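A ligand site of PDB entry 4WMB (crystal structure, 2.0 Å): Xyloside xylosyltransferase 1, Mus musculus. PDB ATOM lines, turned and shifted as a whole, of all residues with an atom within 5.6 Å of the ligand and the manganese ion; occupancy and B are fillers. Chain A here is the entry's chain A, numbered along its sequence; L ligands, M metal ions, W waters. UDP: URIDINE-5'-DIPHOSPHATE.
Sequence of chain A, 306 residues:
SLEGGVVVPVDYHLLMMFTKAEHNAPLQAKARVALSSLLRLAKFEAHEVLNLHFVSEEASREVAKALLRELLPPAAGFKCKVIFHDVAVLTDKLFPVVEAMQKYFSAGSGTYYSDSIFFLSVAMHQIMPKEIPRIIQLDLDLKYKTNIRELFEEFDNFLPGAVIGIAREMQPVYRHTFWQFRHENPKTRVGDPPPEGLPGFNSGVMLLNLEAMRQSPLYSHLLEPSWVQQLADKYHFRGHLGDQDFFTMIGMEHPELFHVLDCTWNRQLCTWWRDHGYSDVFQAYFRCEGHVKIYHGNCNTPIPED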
ATOM      1  N   MET A  16      21.883  30.640  -9.991  1.00  0.00           N
ATOM      2  CA  MET A  16      20.828  29.666 -10.240  1.00  0.00           C
ATOM      3  C   MET A  16      21.263  28.291  -9.738  1.00  0.00           C
ATOM      4  O   MET A  16      22.421  27.867  -9.950  1.00  0.00           O
ATOM      5  CB  MET A  16      20.478  29.626 -11.728  1.00  0.00           C
ATOM      6  CG  MET A  16      19.877  30.932 -12.238  1.00  0.00           C
ATOM      7  SD  MET A  16      20.016  31.121 -14.023  1.00  0.00           S
ATOM      8  CE  MET A  16      19.974  32.908 -14.223  1.00  0.00           C
ATOM      9  N   MET A  17      20.333  27.610  -9.086  1.00  0.00           N
ATOM     10  CA  MET A  17      20.493  26.218  -8.698  1.00  0.00           C
ATOM     11  C   MET A  17      20.285  25.335  -9.921  1.00  0.00           C
ATOM     12  O   MET A  17      19.282  25.485 -10.620  1.00  0.00           O
ATOM     13  CB  MET A  17      19.440  25.869  -7.640  1.00  0.00           C
ATOM     14  CG  MET A  17      19.626  26.602  -6.326  1.00  0.00           C
ATOM     15  SD  MET A  17      21.095  25.922  -5.530  1.00  0.00           S
ATOM     16  CE  MET A  17      20.694  24.151  -5.643  1.00  0.00           C
ATOM     17  N   PHE A  18      21.216  24.430 -10.200  1.00  0.00           N
ATOM     18  CA  PHE A  18      21.019  23.527 -11.353  1.00  0.00           C
ATOM     19  C   PHE A  18      21.643  22.174 -11.047  1.00  0.00           C
ATOM     20  O   PHE A  18      22.802  21.935 -11.368  1.00  0.00           O
ATOM     21  CB  PHE A  18      21.630  24.119 -12.625  1.00  0.00           C
ATOM     22  CG  PHE A  18      21.267  23.366 -13.883  1.00  0.00           C
ATOM     23  CD1 PHE A  18      19.930  23.251 -14.292  1.00  0.00           C
ATOM     24  CD2 PHE A  18      22.255  22.774 -14.664  1.00  0.00           C
ATOM     25  CE1 PHE A  18      19.602  22.574 -15.464  1.00  0.00           C
ATOM     26  CE2 PHE A  18      21.927  22.097 -15.836  1.00  0.00           C
ATOM     27  CZ  PHE A  18      20.592  21.996 -16.244  1.00  0.00           C
ATOM     28  N   THR A  19      20.873  21.320 -10.381  1.00  0.00           N
ATOM     29  CA  THR A  19      21.367  20.068  -9.835  1.00  0.00           C
ATOM     30  C   THR A  19      20.504  18.902 -10.319  1.00  0.00           C
ATOM     31  O   THR A  19      19.325  19.079 -10.671  1.00  0.00           O
ATOM     32  CB  THR A  19      21.324  20.086  -8.289  1.00  0.00           C
ATOM     33  OG1 THR A  19      19.988  20.405  -7.871  1.00  0.00           O
ATOM     34  CG2 THR A  19      22.297  21.118  -7.685  1.00  0.00           C
ATOM     35  N   LYS A  20      21.074  17.694 -10.303  1.00  0.00           N
ATOM     36  CA  LYS A  20      20.366  16.483 -10.728  1.00  0.00           C
ATOM     37  C   LYS A  20      19.757  16.653 -12.136  1.00  0.00           C
ATOM     38  O   LYS A  20      18.650  16.187 -12.410  1.00  0.00           O
ATOM     39  CB  LYS A  20      19.273  16.099  -9.704  1.00  0.00           C
ATOM     40  CG  LYS A  20      19.735  15.983  -8.251  1.00  0.00           C
ATOM     41  CD  LYS A  20      20.799  14.893  -8.099  1.00  0.00           C
ATOM     42  CE  LYS A  20      21.295  14.764  -6.667  1.00  0.00           C
ATOM     43  NZ  LYS A  20      20.251  14.309  -5.707  1.00  0.00           N
ATOM     44  N   ASN A  24      17.350  14.363 -16.900  1.00  0.00           N
ATOM     45  CA  ASN A  24      16.171  15.053 -16.410  1.00  0.00           C
ATOM     46  C   ASN A  24      15.769  16.099 -17.443  1.00  0.00           C
ATOM     47  O   ASN A  24      16.130  17.280 -17.341  1.00  0.00           O
ATOM     48  CB  ASN A  24      16.414  15.665 -15.032  1.00  0.00           C
ATOM     49  CG  ASN A  24      15.199  16.389 -14.480  1.00  0.00           C
ATOM     50  OD1 ASN A  24      14.214  16.615 -15.169  1.00  0.00           O
ATOM     51  ND2 ASN A  24      15.280  16.762 -13.220  1.00  0.00           N
ATOM     52  N   LEU A  27      13.715  19.410 -16.501  1.00  0.00           N
ATOM     53  CA  LEU A  27      14.587  20.456 -15.941  1.00  0.00           C
ATOM     54  C   LEU A  27      15.448  21.144 -16.999  1.00  0.00           C
ATOM     55  O   LEU A  27      15.553  22.371 -17.018  1.00  0.00           O
ATOM     56  CB  LEU A  27      15.477  19.899 -14.814  1.00  0.00           C
ATOM     57  CG  LEU A  27      16.370  20.934 -14.082  1.00  0.00           C
ATOM     58  CD1 LEU A  27      15.534  21.960 -13.325  1.00  0.00           C
ATOM     59  CD2 LEU A  27      17.340  20.247 -13.141  1.00  0.00           C
ATOM     60  N   LYS A  30      13.327  23.487 -19.050  1.00  0.00           N
ATOM     61  CA  LYS A  30      13.074  24.675 -18.231  1.00  0.00           C
ATOM     62  C   LYS A  30      14.276  25.610 -18.259  1.00  0.00           C
ATOM     63  O   LYS A  30      14.144  26.812 -18.519  1.00  0.00           O
ATOM     64  CB  LYS A  30      12.762  24.280 -16.805  1.00  0.00           C
ATOM     65  CG  LYS A  30      11.322  23.907 -16.577  1.00  0.00           C
ATOM     66  CD  LYS A  30      11.193  23.229 -15.226  1.00  0.00           C
ATOM     67  CE  LYS A  30       9.750  22.869 -14.979  1.00  0.00           C
ATOM     68  NZ  LYS A  30       9.616  22.264 -13.619  1.00  0.00           N
ATOM     69  N   PHE A 118      18.818  23.902  -0.020  1.00  0.00           N
ATOM     70  CA  PHE A 118      17.576  24.674  -0.209  1.00  0.00           C
ATOM     71  C   PHE A 118      17.540  25.904   0.702  1.00  0.00           C
ATOM     72  O   PHE A 118      16.640  26.724   0.620  1.00  0.00           O
ATOM     73  CB  PHE A 118      16.314  23.789  -0.078  1.00  0.00           C
ATOM     74  CG  PHE A 118      16.294  22.637  -1.058  1.00  0.00           C
ATOM     75  CD1 PHE A 118      16.338  22.878  -2.433  1.00  0.00           C
ATOM     76  CD2 PHE A 118      16.294  21.323  -0.610  1.00  0.00           C
ATOM     77  CE1 PHE A 118      16.359  21.824  -3.349  1.00  0.00           C
ATOM     78  CE2 PHE A 118      16.308  20.255  -1.511  1.00  0.00           C
ATOM     79  CZ  PHE A 118      16.343  20.505  -2.888  1.00  0.00           C
ATOM     80  N   LEU A 138      17.911  33.178  -8.839  1.00  0.00           N
ATOM     81  CA  LEU A 138      16.807  32.975  -9.759  1.00  0.00           C
ATOM     82  C   LEU A 138      16.506  31.490  -9.908  1.00  0.00           C
ATOM     83  O   LEU A 138      17.422  30.675 -10.013  1.00  0.00           O
ATOM     84  CB  LEU A 138      17.137  33.602 -11.129  1.00  0.00           C
ATOM     85  CG  LEU A 138      17.347  35.122 -11.063  1.00  0.00           C
ATOM     86  CD1 LEU A 138      18.202  35.692 -12.199  1.00  0.00           C
ATOM     87  CD2 LEU A 138      16.000  35.823 -10.957  1.00  0.00           C
ATOM     88  N   ASP A 139      15.216  31.119  -9.909  1.00  0.00           N
ATOM     89  CA  ASP A 139      14.817  29.770 -10.318  1.00  0.00           C
ATOM     90  C   ASP A 139      15.077  29.558 -11.805  1.00  0.00           C
ATOM     91  O   ASP A 139      15.320  30.528 -12.538  1.00  0.00           O
ATOM     92  CB  ASP A 139      13.347  29.551 -10.038  1.00  0.00           C
ATOM     93  CG  ASP A 139      13.114  29.135  -8.621  1.00  0.00           C
ATOM     94  OD1 ASP A 139      14.085  29.216  -7.825  1.00  0.00           O
ATOM     95  OD2 ASP A 139      11.990  28.728  -8.315  1.00  0.00           O
ATOM     96  N   LEU A 140      15.040  28.301 -12.246  1.00  0.00           N
ATOM     97  CA  LEU A 140      15.233  28.020 -13.679  1.00  0.00           C
ATOM     98  C   LEU A 140      13.916  27.735 -14.439  1.00  0.00           C
ATOM     99  O   LEU A 140      13.914  27.547 -15.661  1.00  0.00           O
ATOM    100  CB  LEU A 140      16.296  26.923 -13.898  1.00  0.00           C
ATOM    101  CG  LEU A 140      17.738  27.490 -13.925  1.00  0.00           C
ATOM    102  CD1 LEU A 140      18.824  26.444 -13.739  1.00  0.00           C
ATOM    103  CD2 LEU A 140      18.005  28.290 -15.199  1.00  0.00           C
ATOM    104  N   ASP A 141      12.804  27.697 -13.703  1.00  0.00           N
ATOM    105  CA  ASP A 141      11.478  27.545 -14.318  1.00  0.00           C
ATOM    106  C   ASP A 141      10.841  28.933 -14.562  1.00  0.00           C
ATOM    107  O   ASP A 141       9.645  29.140 -14.322  1.00  0.00           O
ATOM    108  CB  ASP A 141      10.567  26.616 -13.480  1.00  0.00           C
ATOM    109  CG  ASP A 141      10.290  27.144 -12.065  1.00  0.00           C
ATOM    110  OD1 ASP A 141      11.116  27.895 -11.491  1.00  0.00           O
ATOM    111  OD2 ASP A 141       9.224  26.787 -11.487  1.00  0.00           O
ATOM    112  N   LEU A 142      11.677  29.848 -15.056  1.00  0.00           N
ATOM    113  CA  LEU A 142      11.297  31.233 -15.335  1.00  0.00           C
ATOM    114  C   LEU A 142      11.299  31.516 -16.841  1.00  0.00           C
ATOM    115  O   LEU A 142      11.888  30.768 -17.629  1.00  0.00           O
ATOM    116  CB  LEU A 142      12.262  32.198 -14.637  1.00  0.00           C
ATOM    117  CG  LEU A 142      12.491  32.145 -13.115  1.00  0.00           C
ATOM    118  CD1 LEU A 142      13.383  33.292 -12.658  1.00  0.00           C
ATOM    119  CD2 LEU A 142      11.177  32.224 -12.361  1.00  0.00           C
ATOM    120  N   GLY A 204      11.420  32.441  -5.979  1.00  0.00           N
ATOM    121  CA  GLY A 204      11.825  32.263  -7.387  1.00  0.00           C
ATOM    122  C   GLY A 204      12.712  33.385  -7.893  1.00  0.00           C
ATOM    123  O   GLY A 204      13.484  33.169  -8.811  1.00  0.00           O
ATOM    124  N   LEU A 241       9.478  24.092   2.128  1.00  0.00           N
ATOM    125  CA  LEU A 241       9.961  24.939   1.029  1.00  0.00           C
ATOM    126  C   LEU A 241      11.243  25.738   1.328  1.00  0.00           C
ATOM    127  O   LEU A 241      11.621  26.614   0.536  1.00  0.00           O
ATOM    128  CB  LEU A 241       8.830  25.834   0.480  1.00  0.00           C
ATOM    129  CG  LEU A 241       7.608  25.038   0.000  1.00  0.00           C
ATOM    130  CD1 LEU A 241       6.456  25.966  -0.364  1.00  0.00           C
ATOM    131  CD2 LEU A 241       8.012  24.168  -1.188  1.00  0.00           C
ATOM    132  N   GLN A 244      12.440  29.901   1.258  1.00  0.00           N
ATOM    133  CA  GLN A 244      11.142  30.560   1.115  1.00  0.00           C
ATOM    134  C   GLN A 244      10.390  30.597   2.446  1.00  0.00           C
ATOM    135  O   GLN A 244       9.897  31.638   2.845  1.00  0.00           O
ATOM    136  CB  GLN A 244      10.313  29.828   0.075  1.00  0.00           C
ATOM    137  CG  GLN A 244       9.038  30.539  -0.229  1.00  0.00           C
ATOM    138  CD  GLN A 244       8.309  29.929  -1.376  1.00  0.00           C
ATOM    139  OE1 GLN A 244       8.813  29.901  -2.479  1.00  0.00           O
ATOM    140  NE2 GLN A 244       7.092  29.440  -1.105  1.00  0.00           N
ATOM    141  N   HIS A 296       6.935  32.930 -13.807  1.00  0.00           N
ATOM    142  CA  HIS A 296       7.441  31.838 -12.990  1.00  0.00           C
ATOM    143  C   HIS A 296       6.482  30.705 -13.118  1.00  0.00           C
ATOM    144  O   HIS A 296       5.407  30.716 -12.504  1.00  0.00           O
ATOM    145  CB  HIS A 296       7.579  32.301 -11.537  1.00  0.00           C
ATOM    146  CG  HIS A 296       8.228  31.300 -10.589  1.00  0.00           C
ATOM    147  ND1 HIS A 296       8.342  31.535  -9.266  1.00  0.00           N
ATOM    148  CD2 HIS A 296       8.802  30.043 -10.821  1.00  0.00           C
ATOM    149  CE1 HIS A 296       8.955  30.475  -8.666  1.00  0.00           C
ATOM    150  NE2 HIS A 296       9.236  29.561  -9.617  1.00  0.00           N
ATOM    151  N   GLY A 297       6.866  29.707 -13.904  1.00  0.00           N
ATOM    152  CA  GLY A 297       6.066  28.498 -14.120  1.00  0.00           C
ATOM    153  C   GLY A 297       6.224  27.487 -13.001  1.00  0.00           C
ATOM    154  O   GLY A 297       6.581  26.329 -13.250  1.00  0.00           O
ATOM    155  N   ASN A 298       5.938  27.909 -11.761  1.00  0.00           N
ATOM    156  CA  ASN A 298       6.127  27.007 -10.611  1.00  0.00           C
ATOM    157  C   ASN A 298       5.167  25.819 -10.631  1.00  0.00           C
ATOM    158  O   ASN A 298       4.234  25.788 -11.437  1.00  0.00           O
ATOM    159  CB  ASN A 298       6.214  27.734  -9.240  1.00  0.00           C
ATOM    160  CG  ASN A 298       4.994  28.612  -8.911  1.00  0.00           C
ATOM    161  OD1 ASN A 298       4.739  28.900  -7.727  1.00  0.00           O
ATOM    162  ND2 ASN A 298       4.265  29.054  -9.906  1.00  0.00           N
ATOM    163  N   CYS A 299       5.428  24.836  -9.766  1.00  0.00           N
ATOM    164  CA  CYS A 299       4.771  23.520  -9.790  1.00  0.00           C
ATOM    165  C   CYS A 299       4.566  22.981 -11.211  1.00  0.00           C
ATOM    166  O   CYS A 299       3.480  22.522 -11.575  1.00  0.00           O
ATOM    167  CB  CYS A 299       3.488  23.480  -8.932  1.00  0.00           C
ATOM    168  SG  CYS A 299       1.971  24.216  -9.622  1.00  0.00           S
ATOM    169  N   ASN A 300       5.626  23.067 -12.021  1.00  0.00           N
ATOM    170  CA  ASN A 300       5.653  22.497 -13.363  1.00  0.00           C
ATOM    171  C   ASN A 300       4.549  23.013 -14.266  1.00  0.00           C
ATOM    172  O   ASN A 300       4.089  22.299 -15.144  1.00  0.00           O
ATOM    173  CB  ASN A 300       5.554  20.972 -13.280  1.00  0.00           C
ATOM    174  CG  ASN A 300       6.743  20.347 -12.587  1.00  0.00           C
ATOM    175  OD1 ASN A 300       7.864  20.718 -12.858  1.00  0.00           O
ATOM    176  ND2 ASN A 300       6.488  19.409 -11.703  1.00  0.00           N
HETATM  177  N1  UDP L   1      16.189  22.683  -9.089  1.00  0.00           N
HETATM  178  C2  UDP L   1      17.259  21.935  -9.614  1.00  0.00           C
HETATM  179  N3  UDP L   1      17.172  20.601  -9.697  1.00  0.00           N
HETATM  180  C4  UDP L   1      16.073  19.962  -9.281  1.00  0.00           C
HETATM  181  C5  UDP L   1      14.987  20.662  -8.748  1.00  0.00           C
HETATM  182  C6  UDP L   1      15.076  22.046  -8.653  1.00  0.00           C
HETATM  183  O2  UDP L   1      18.290  22.521  -9.988  1.00  0.00           O
HETATM  184  O4  UDP L   1      16.022  18.723  -9.367  1.00  0.00           O
HETATM  185  C1' UDP L   1      16.325  24.151  -8.995  1.00  0.00           C
HETATM  186  C2' UDP L   1      15.808  24.872 -10.211  1.00  0.00           C
HETATM  187  O2' UDP L   1      16.640  26.026 -10.368  1.00  0.00           O
HETATM  188  C3' UDP L   1      14.397  25.278  -9.803  1.00  0.00           C
HETATM  189  C4' UDP L   1      14.543  25.558  -8.305  1.00  0.00           C
HETATM  190  O4' UDP L   1      15.557  24.653  -7.888  1.00  0.00           O
HETATM  191  O3' UDP L   1      13.918  26.411 -10.511  1.00  0.00           O
HETATM  192  C5' UDP L   1      13.298  25.339  -7.465  1.00  0.00           C
HETATM  193  O5' UDP L   1      12.572  24.198  -7.944  1.00  0.00           O
HETATM  194  PA  UDP L   1      11.229  24.419  -8.799  1.00  0.00           P
HETATM  195  O1A UDP L   1      11.359  25.713  -9.546  1.00  0.00           O
HETATM  196  O2A UDP L   1      10.884  23.175  -9.564  1.00  0.00           O
HETATM  197  O3A UDP L   1      10.188  24.549  -7.556  1.00  0.00           O
HETATM  198  PB  UDP L   1       8.910  25.527  -7.506  1.00  0.00           P
HETATM  199  O1B UDP L   1       8.747  25.758  -6.029  1.00  0.00           O
HETATM  200  O2B UDP L   1       7.775  24.754  -8.083  1.00  0.00           O
HETATM  201  O3B UDP L   1       9.289  26.784  -8.295  1.00  0.00           O
HETATM  202 MN    MN M   1      10.347  27.738  -9.555  1.00  0.00          MN
HETATM  203  O   HOH W   1      17.776  28.453  -8.863  1.00  0.00           O
HETATM  204  O   HOH W   2       8.007  22.225  -8.752  1.00  0.00           O
HETATM  205  O   HOH W   3       8.701  27.798  -3.725  1.00  0.00           O
HETATM  206  O   HOH W   4       8.507  24.134 -11.634  1.00  0.00           O
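Three residues have an atom within 4 Å of the manganese ion: Asp 139, Asp 141 and His 296.
Along chain A the residues within 4 Å of the manganese ion span positions 139 to 296.
The nearest printed residue that does not touch the manganese ion is Asn 298 (4.1 Å).
The manganese ion is bound by an oxygen (O3B) of the ligand, the side-chain carboxylate (OD1) of Asp 141, a ring nitrogen (NE2) of His 296, an oxygen (O1A) of the ligand, the side-chain carboxylate (OD2) of Asp 139 and the side-chain carboxylate (OD2) of Asp 141.
The manganese ion has six donor atoms within binding distance.
O of Met 17 is in hydrogen-bond range of O2' of the ligand, at 2.7 Å.
An oxygen (O3') of the ligand lies within hydrogen-bond range of the backbone NH (N) of Leu 140 (2.8 Å).
The backbone NH (N) of Thr 19 is in hydrogen-bond range of an oxygen (O2) of the ligand (2.9 Å).
A nitrogen (N3) of the ligand lies within hydrogen-bond range of the backbone carbonyl oxygen (O) of Thr 19, 2.8 Å away.
The side-chain hydroxyl of Thr 19 sits at hydrogen-bond distance from a nitrogen (N3) of the ligand, 3.4 Å away.
O2B of the ligand sits at hydrogen-bond distance from N of Cys 299 (2.9 Å).
Phe 18 touches the ligand (CA to O2, 3.2 Å).
Leu 27 touches the ligand (CD2 to N3, 3.5 Å).
Asn 298 touches the ligand (CB to O3B, 3.4 Å).
Hydrophobic or aromatic side chains within 4 Å of the ligand: Met 17, Leu 27, Leu 140 and His 296.
Within 4 Å of the ligand: Met 17, Phe 18, Thr 19, Leu 27, Asp 139, Leu 140, Asp 141, His 296, Asn 298 and Cys 299.
Water W1 lies within hydrogen-bond range of O of Leu 138 (2.5 Å), N of Met 17 (2.7 Å) and O2' of the ligand (3.1 Å).
Water W3 bridges OE1 of Gln 244 (2.4 Å) and O1B of the ligand (3.1 Å).
Water W4 lies within hydrogen-bond range of the side-chain amino group (NZ) of Lys 30 (2.9 Å), the backbone NH (N) of Asn 300 (3.1 Å), an oxygen (O2A) of the ligand (3.3 Å) and the backbone carbonyl oxygen (O) of Gly 297 (3.3 Å).
The backbone NH (N) of Asn 298 lies close to the side-chain carboxylate (OD2) of Asp 141 (3.5 Å).
The backbone carbonyl oxygen of Asp 141 sits at hydrogen-bond distance from the backbone NH of Gly 297 (2.9 Å).
The backbone carbonyl oxygen (O) of His 296 sits at hydrogen-bond distance from the side-chain amide nitrogen (ND2) of Asn 298, at 3.3 Å.
The backbone NH (N) of Asp 139 sits at hydrogen-bond distance from the backbone carbonyl oxygen (O) of Gly 204 (2.9 Å).
The backbone NH (N) of Leu 27 sits at hydrogen-bond distance from the side-chain amide oxygen (OD1) of Asn 24.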
